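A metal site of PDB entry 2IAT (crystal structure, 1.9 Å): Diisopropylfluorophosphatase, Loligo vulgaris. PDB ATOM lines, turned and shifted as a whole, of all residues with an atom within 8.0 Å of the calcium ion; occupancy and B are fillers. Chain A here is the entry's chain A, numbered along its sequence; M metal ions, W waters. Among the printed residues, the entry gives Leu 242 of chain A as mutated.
The backbone carbonyl oxygen (O) of Asn 173 lies within hydrogen-bond range of the side-chain hydroxyl (OG1) of Thr 131 (2.6 Å).
The side-chain amide nitrogen (ND2) of Asn 173 lies within hydrogen-bond range of the side-chain hydroxyl (OG1) of Thr 193 (2.9 Å).
OE2 of Glu 19 sits close to OG of Ser 269 (3.2 Å).
The side-chain carboxylate (OD2) of Asp 227 sits at hydrogen-bond distance from the side-chain hydroxyl (OG) of Ser 269 (2.8 Å).
The backbone carbonyl oxygen of Asp 227 is in hydrogen-bond range of the backbone NH of Gly 174 (2.8 Å).
O of Asn 118 sits at hydrogen-bond distance from N of Gly 73 (3.0 Å).
The backbone NH of Asn 118 lies within hydrogen-bond range of the backbone carbonyl oxygen of Thr 131 (2.9 Å).
ND2 of Asn 118 is in hydrogen-bond range of SD of Met 88 (3.5 Å).
Of the 29 residues printed, 4 come within 4 Å of the calcium ion.
Along chain A the residues within 4 Å of the calcium ion span positions 19 to 227.
The calcium ion is bound by the side-chain amide oxygen (OD1) of Asn 173 (2.4 Å), the side-chain carboxylate (OE2) of Glu 19 (2.4 Å), the side-chain carboxylate (OD1) of Asp 227 (2.5 Å), water W2 (2.5 Å), the side-chain amide oxygen (OD1) of Asn 118 (2.5 Å), water W1 (2.5 Å) and water W3 (2.7 Å).
The calcium ion has seven donor atoms within binding distance.
Water W1 lies within hydrogen-bond range of ND2 of Asn 118 (3.2 Å) and ND2 of Asn 173 (3.4 Å).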
ATOM      1  N   GLY A  17      -3.887  19.230  20.415  1.00  0.00           N
ATOM      2  CA  GLY A  17      -5.055  18.797  21.159  1.00  0.00           C
ATOM      3  C   GLY A  17      -5.031  17.329  21.544  1.00  0.00           C
ATOM      4  O   GLY A  17      -6.098  16.758  21.775  1.00  0.00           O
ATOM      5  N   ALA A  18      -3.824  16.747  21.645  1.00  0.00           N
ATOM      6  CA  ALA A  18      -3.620  15.326  21.993  1.00  0.00           C
ATOM      7  C   ALA A  18      -4.746  14.789  22.873  1.00  0.00           C
ATOM      8  O   ALA A  18      -4.881  15.181  24.029  1.00  0.00           O
ATOM      9  CB  ALA A  18      -2.274  15.148  22.697  1.00  0.00           C
ATOM     10  N   GLU A  19      -5.548  13.899  22.312  1.00  0.00           N
ATOM     11  CA  GLU A  19      -6.693  13.334  23.002  1.00  0.00           C
ATOM     12  C   GLU A  19      -6.963  11.883  22.637  1.00  0.00           C
ATOM     13  O   GLU A  19      -6.243  11.283  21.830  1.00  0.00           O
ATOM     14  CB  GLU A  19      -7.937  14.143  22.631  1.00  0.00           C
ATOM     15  CG  GLU A  19      -8.424  15.095  23.700  1.00  0.00           C
ATOM     16  CD  GLU A  19      -9.349  14.433  24.693  1.00  0.00           C
ATOM     17  OE1 GLU A  19      -9.380  13.176  24.762  1.00  0.00           O
ATOM     18  OE2 GLU A  19     -10.057  15.168  25.392  1.00  0.00           O
ATOM     19  N   GLY A  20      -8.028  11.356  23.226  1.00  0.00           N
ATOM     20  CA  GLY A  20      -8.492  10.004  22.990  1.00  0.00           C
ATOM     21  C   GLY A  20      -7.513   8.836  22.896  1.00  0.00           C
ATOM     22  O   GLY A  20      -7.668   8.014  21.995  1.00  0.00           O
ATOM     23  N   PRO A  34      -7.504  16.391  17.630  1.00  0.00           N
ATOM     24  CA  PRO A  34      -8.671  17.191  17.251  1.00  0.00           C
ATOM     25  C   PRO A  34      -8.401  18.605  16.769  1.00  0.00           C
ATOM     26  O   PRO A  34      -9.007  19.057  15.802  1.00  0.00           O
ATOM     27  CB  PRO A  34      -9.505  17.204  18.537  1.00  0.00           C
ATOM     28  CG  PRO A  34      -8.482  17.053  19.618  1.00  0.00           C
ATOM     29  CD  PRO A  34      -7.571  16.013  19.048  1.00  0.00           C
ATOM     30  N   ALA A  72     -12.064  13.578  18.962  1.00  0.00           N
ATOM     31  CA  ALA A  72     -11.638  13.854  20.323  1.00  0.00           C
ATOM     32  C   ALA A  72     -11.544  12.696  21.321  1.00  0.00           C
ATOM     33  O   ALA A  72     -10.861  12.832  22.334  1.00  0.00           O
ATOM     34  CB  ALA A  72     -12.500  14.973  20.909  1.00  0.00           C
ATOM     35  N   GLY A  73     -12.237  11.595  21.049  1.00  0.00           N
ATOM     36  CA  GLY A  73     -12.208  10.460  21.964  1.00  0.00           C
ATOM     37  C   GLY A  73     -12.334   9.115  21.256  1.00  0.00           C
ATOM     38  O   GLY A  73     -12.942   9.024  20.186  1.00  0.00           O
ATOM     39  N   MET A  88     -16.239  16.015  17.429  1.00  0.00           N
ATOM     40  CA  MET A  88     -16.960  17.255  17.766  1.00  0.00           C
ATOM     41  C   MET A  88     -17.728  17.885  16.591  1.00  0.00           C
ATOM     42  O   MET A  88     -18.663  18.650  16.802  1.00  0.00           O
ATOM     43  CB  MET A  88     -15.998  18.272  18.394  1.00  0.00           C
ATOM     44  CG  MET A  88     -15.452  17.868  19.775  1.00  0.00           C
ATOM     45  SD  MET A  88     -16.716  17.923  21.058  1.00  0.00           S
ATOM     46  CE  MET A  88     -16.739  19.679  21.430  1.00  0.00           C
ATOM     47  N   CYS A 117     -19.687  14.840  19.160  1.00  0.00           N
ATOM     48  CA  CYS A 117     -19.318  14.055  20.322  1.00  0.00           C
ATOM     49  C   CYS A 117     -17.874  14.295  20.769  1.00  0.00           C
ATOM     50  O   CYS A 117     -17.043  14.778  20.009  1.00  0.00           O
ATOM     51  CB  CYS A 117     -19.610  12.588  20.043  1.00  0.00           C
ATOM     52  SG  CYS A 117     -21.392  12.267  19.779  1.00  0.00           S
ATOM     53  N   ASN A 118     -17.586  13.970  22.033  1.00  0.00           N
ATOM     54  CA  ASN A 118     -16.258  14.204  22.564  1.00  0.00           C
ATOM     55  C   ASN A 118     -15.547  12.963  23.088  1.00  0.00           C
ATOM     56  O   ASN A 118     -14.345  12.778  22.855  1.00  0.00           O
ATOM     57  CB  ASN A 118     -16.326  15.270  23.654  1.00  0.00           C
ATOM     58  CG  ASN A 118     -14.979  15.713  24.102  1.00  0.00           C
ATOM     59  OD1 ASN A 118     -14.363  15.069  24.947  1.00  0.00           O
ATOM     60  ND2 ASN A 118     -14.482  16.794  23.515  1.00  0.00           N
ATOM     61  N   ASP A 119     -16.264  12.132  23.841  1.00  0.00           N
ATOM     62  CA  ASP A 119     -15.694  10.907  24.378  1.00  0.00           C
ATOM     63  C   ASP A 119     -16.778   9.830  24.475  1.00  0.00           C
ATOM     64  O   ASP A 119     -17.969  10.132  24.421  1.00  0.00           O
ATOM     65  CB  ASP A 119     -15.046  11.142  25.749  1.00  0.00           C
ATOM     66  CG  ASP A 119     -13.807  10.263  25.985  1.00  0.00           C
ATOM     67  OD1 ASP A 119     -13.583   9.301  25.220  1.00  0.00           O
ATOM     68  OD2 ASP A 119     -13.045  10.544  26.933  1.00  0.00           O
ATOM     69  N   CYS A 120     -16.349   8.586  24.593  1.00  0.00           N
ATOM     70  CA  CYS A 120     -17.271   7.453  24.700  1.00  0.00           C
ATOM     71  C   CYS A 120     -16.701   6.312  25.525  1.00  0.00           C
ATOM     72  O   CYS A 120     -15.482   6.224  25.734  1.00  0.00           O
ATOM     73  CB  CYS A 120     -17.653   6.945  23.310  1.00  0.00           C
ATOM     74  SG  CYS A 120     -16.262   6.525  22.252  1.00  0.00           S
ATOM     75  N   THR A 131     -20.538  11.150  25.100  1.00  0.00           N
ATOM     76  CA  THR A 131     -20.791  12.528  25.511  1.00  0.00           C
ATOM     77  C   THR A 131     -20.842  13.422  24.268  1.00  0.00           C
ATOM     78  O   THR A 131     -20.036  13.274  23.348  1.00  0.00           O
ATOM     79  CB  THR A 131     -19.707  13.063  26.460  1.00  0.00           C
ATOM     80  OG1 THR A 131     -18.405  12.848  25.897  1.00  0.00           O
ATOM     81  CG2 THR A 131     -19.829  12.406  27.817  1.00  0.00           C
ATOM     82  N   PRO A 133     -20.866  17.282  23.840  1.00  0.00           N
ATOM     83  CA  PRO A 133     -20.767  18.673  24.300  1.00  0.00           C
ATOM     84  C   PRO A 133     -20.922  19.731  23.196  1.00  0.00           C
ATOM     85  O   PRO A 133     -21.116  20.911  23.482  1.00  0.00           O
ATOM     86  CB  PRO A 133     -19.378  18.732  24.921  1.00  0.00           C
ATOM     87  CG  PRO A 133     -18.609  17.776  24.078  1.00  0.00           C
ATOM     88  CD  PRO A 133     -19.556  16.608  23.933  1.00  0.00           C
ATOM     89  N   PHE A 171     -21.021  21.107  28.927  1.00  0.00           N
ATOM     90  CA  PHE A 171     -19.847  20.440  28.377  1.00  0.00           C
ATOM     91  C   PHE A 171     -19.584  19.047  28.942  1.00  0.00           C
ATOM     92  O   PHE A 171     -18.677  18.865  29.745  1.00  0.00           O
ATOM     93  CB  PHE A 171     -18.586  21.315  28.466  1.00  0.00           C
ATOM     94  CG  PHE A 171     -17.580  21.009  27.372  1.00  0.00           C
ATOM     95  CD1 PHE A 171     -16.641  19.995  27.535  1.00  0.00           C
ATOM     96  CD2 PHE A 171     -17.601  21.724  26.176  1.00  0.00           C
ATOM     97  CE1 PHE A 171     -15.737  19.689  26.506  1.00  0.00           C
ATOM     98  CE2 PHE A 171     -16.712  21.419  25.150  1.00  0.00           C
ATOM     99  CZ  PHE A 171     -15.773  20.406  25.313  1.00  0.00           C
ATOM    100  N   PRO A 172     -20.457  18.074  28.596  1.00  0.00           N
ATOM    101  CA  PRO A 172     -20.280  16.696  29.074  1.00  0.00           C
ATOM    102  C   PRO A 172     -18.960  16.262  28.412  1.00  0.00           C
ATOM    103  O   PRO A 172     -18.724  16.537  27.228  1.00  0.00           O
ATOM    104  CB  PRO A 172     -21.511  15.980  28.507  1.00  0.00           C
ATOM    105  CG  PRO A 172     -21.907  16.797  27.332  1.00  0.00           C
ATOM    106  CD  PRO A 172     -21.698  18.202  27.825  1.00  0.00           C
ATOM    107  N   ASN A 173     -18.080  15.632  29.186  1.00  0.00           N
ATOM    108  CA  ASN A 173     -16.771  15.302  28.665  1.00  0.00           C
ATOM    109  C   ASN A 173     -16.414  13.831  28.783  1.00  0.00           C
ATOM    110  O   ASN A 173     -16.833  13.018  27.972  1.00  0.00           O
ATOM    111  CB  ASN A 173     -15.735  16.179  29.361  1.00  0.00           C
ATOM    112  CG  ASN A 173     -14.542  16.477  28.491  1.00  0.00           C
ATOM    113  OD1 ASN A 173     -14.091  15.619  27.745  1.00  0.00           O
ATOM    114  ND2 ASN A 173     -14.029  17.690  28.582  1.00  0.00           N
ATOM    115  N   GLY A 174     -15.610  13.498  29.796  1.00  0.00           N
ATOM    116  CA  GLY A 174     -15.225  12.119  29.998  1.00  0.00           C
ATOM    117  C   GLY A 174     -16.437  11.303  30.394  1.00  0.00           C
ATOM    118  O   GLY A 174     -17.427  11.841  30.886  1.00  0.00           O
ATOM    119  N   ILE A 175     -16.348  10.001  30.174  1.00  0.00           N
ATOM    120  CA  ILE A 175     -17.427   9.079  30.498  1.00  0.00           C
ATOM    121  C   ILE A 175     -16.827   7.702  30.721  1.00  0.00           C
ATOM    122  O   ILE A 175     -15.852   7.334  30.071  1.00  0.00           O
ATOM    123  CB  ILE A 175     -18.508   9.075  29.362  1.00  0.00           C
ATOM    124  CG1 ILE A 175     -19.717   8.228  29.754  1.00  0.00           C
ATOM    125  CG2 ILE A 175     -17.906   8.603  28.046  1.00  0.00           C
ATOM    126  CD1 ILE A 175     -20.918   8.446  28.868  1.00  0.00           C
ATOM    127  N   THR A 193     -17.248  19.175  32.721  1.00  0.00           N
ATOM    128  CA  THR A 193     -16.040  19.971  32.926  1.00  0.00           C
ATOM    129  C   THR A 193     -16.058  21.247  33.760  1.00  0.00           C
ATOM    130  O   THR A 193     -15.631  21.236  34.903  1.00  0.00           O
ATOM    131  CB  THR A 193     -15.262  20.193  31.613  1.00  0.00           C
ATOM    132  OG1 THR A 193     -15.158  18.947  30.903  1.00  0.00           O
ATOM    133  CG2 THR A 193     -13.859  20.705  31.888  1.00  0.00           C
ATOM    134  N   ALA A 226     -12.756  18.101  35.072  1.00  0.00           N
ATOM    135  CA  ALA A 226     -12.724  16.708  34.615  1.00  0.00           C
ATOM    136  C   ALA A 226     -12.822  16.559  33.103  1.00  0.00           C
ATOM    137  O   ALA A 226     -13.786  16.996  32.475  1.00  0.00           O
ATOM    138  CB  ALA A 226     -13.846  15.894  35.289  1.00  0.00           C
ATOM    139  N   ASP A 227     -11.822  15.908  32.544  1.00  0.00           N
ATOM    140  CA  ASP A 227     -11.762  15.704  31.102  1.00  0.00           C
ATOM    141  C   ASP A 227     -11.923  14.207  30.843  1.00  0.00           C
ATOM    142  O   ASP A 227     -13.031  13.686  30.975  1.00  0.00           O
ATOM    143  CB  ASP A 227     -10.437  16.245  30.573  1.00  0.00           C
ATOM    144  CG  ASP A 227     -10.431  16.392  29.067  1.00  0.00           C
ATOM    145  OD1 ASP A 227     -11.225  15.709  28.404  1.00  0.00           O
ATOM    146  OD2 ASP A 227      -9.620  17.176  28.533  1.00  0.00           O
ATOM    147  N   GLY A 228     -10.838  13.504  30.535  1.00  0.00           N
ATOM    148  CA  GLY A 228     -10.923  12.073  30.289  1.00  0.00           C
ATOM    149  C   GLY A 228     -10.971  11.289  31.588  1.00  0.00           C
ATOM    150  O   GLY A 228     -10.560  11.812  32.628  1.00  0.00           O
ATOM    151  N   MET A 229     -11.444  10.038  31.545  1.00  0.00           N
ATOM    152  CA  MET A 229     -11.523   9.179  32.729  1.00  0.00           C
ATOM    153  C   MET A 229     -11.538   7.687  32.397  1.00  0.00           C
ATOM    154  O   MET A 229     -11.957   7.280  31.314  1.00  0.00           O
ATOM    155  CB  MET A 229     -12.794   9.498  33.535  1.00  0.00           C
ATOM    156  CG  MET A 229     -14.078   9.132  32.831  1.00  0.00           C
ATOM    157  SD  MET A 229     -15.545   9.258  33.840  1.00  0.00           S
ATOM    158  CE  MET A 229     -15.437  10.948  34.339  1.00  0.00           C
ATOM    159  N   LEU A 242      -8.051  18.736  34.017  1.00  0.00           N
ATOM    160  CA  LEU A 242      -7.358  19.721  33.190  1.00  0.00           C
ATOM    161  C   LEU A 242      -7.249  21.088  33.833  1.00  0.00           C
ATOM    162  O   LEU A 242      -8.247  21.686  34.247  1.00  0.00           O
ATOM    163  CB  LEU A 242      -8.022  19.831  31.807  1.00  0.00           C
ATOM    164  CG  LEU A 242      -7.249  20.675  30.771  1.00  0.00           C
ATOM    165  CD1 LEU A 242      -7.248  19.982  29.420  1.00  0.00           C
ATOM    166  CD2 LEU A 242      -7.856  22.073  30.685  1.00  0.00           C
ATOM    167  N   SER A 269      -5.219  15.779  29.905  1.00  0.00           N
ATOM    168  CA  SER A 269      -6.484  15.746  29.189  1.00  0.00           C
ATOM    169  C   SER A 269      -7.206  14.411  29.231  1.00  0.00           C
ATOM    170  O   SER A 269      -8.339  14.320  29.704  1.00  0.00           O
ATOM    171  CB  SER A 269      -6.250  16.173  27.738  1.00  0.00           C
ATOM    172  OG  SER A 269      -7.467  16.185  27.021  1.00  0.00           O
ATOM    173  N   ASN A 270      -6.564  13.358  28.740  1.00  0.00           N
ATOM    174  CA  ASN A 270      -7.209  12.060  28.738  1.00  0.00           C
ATOM    175  C   ASN A 270      -6.164  11.006  29.103  1.00  0.00           C
ATOM    176  O   ASN A 270      -4.962  11.301  29.156  1.00  0.00           O
ATOM    177  CB  ASN A 270      -7.841  11.792  27.361  1.00  0.00           C
ATOM    178  CG  ASN A 270      -9.143  10.967  27.441  1.00  0.00           C
ATOM    179  OD1 ASN A 270     -10.098  11.202  26.692  1.00  0.00           O
ATOM    180  ND2 ASN A 270      -9.166   9.999  28.345  1.00  0.00           N
ATOM    181  N   THR A 283      -2.406  12.122  27.861  1.00  0.00           N
ATOM    182  CA  THR A 283      -2.265  13.178  26.871  1.00  0.00           C
ATOM    183  C   THR A 283      -2.486  14.499  27.596  1.00  0.00           C
ATOM    184  O   THR A 283      -3.307  14.588  28.520  1.00  0.00           O
ATOM    185  CB  THR A 283      -3.296  13.029  25.751  1.00  0.00           C
ATOM    186  OG1 THR A 283      -4.623  13.070  26.298  1.00  0.00           O
ATOM    187  CG2 THR A 283      -3.088  11.710  25.028  1.00  0.00           C
ATOM    188  N   HIS A 285      -2.445  19.080  27.140  1.00  0.00           N
ATOM    189  CA  HIS A 285      -2.572  20.188  26.191  1.00  0.00           C
ATOM    190  C   HIS A 285      -1.621  21.368  26.349  1.00  0.00           C
ATOM    191  O   HIS A 285      -1.737  22.356  25.617  1.00  0.00           O
ATOM    192  CB  HIS A 285      -4.028  20.652  26.157  1.00  0.00           C
ATOM    193  CG  HIS A 285      -4.980  19.629  25.622  1.00  0.00           C
ATOM    194  ND1 HIS A 285      -6.351  19.795  25.624  1.00  0.00           N
ATOM    195  CD2 HIS A 285      -4.751  18.412  25.050  1.00  0.00           C
ATOM    196  CE1 HIS A 285      -6.918  18.741  25.072  1.00  0.00           C
ATOM    197  NE2 HIS A 285      -5.977  17.884  24.726  1.00  0.00           N
HETATM  198 CA    CA M   1     -12.293  14.997  26.295  1.00  0.00          CA
HETATM  199  O   HOH W   1     -12.253  17.444  25.704  1.00  0.00           O
HETATM  200  O   HOH W   2     -12.829  13.012  27.664  1.00  0.00           O
HETATM  201  O   HOH W   3     -12.108  12.835  24.690  1.00  0.00           O
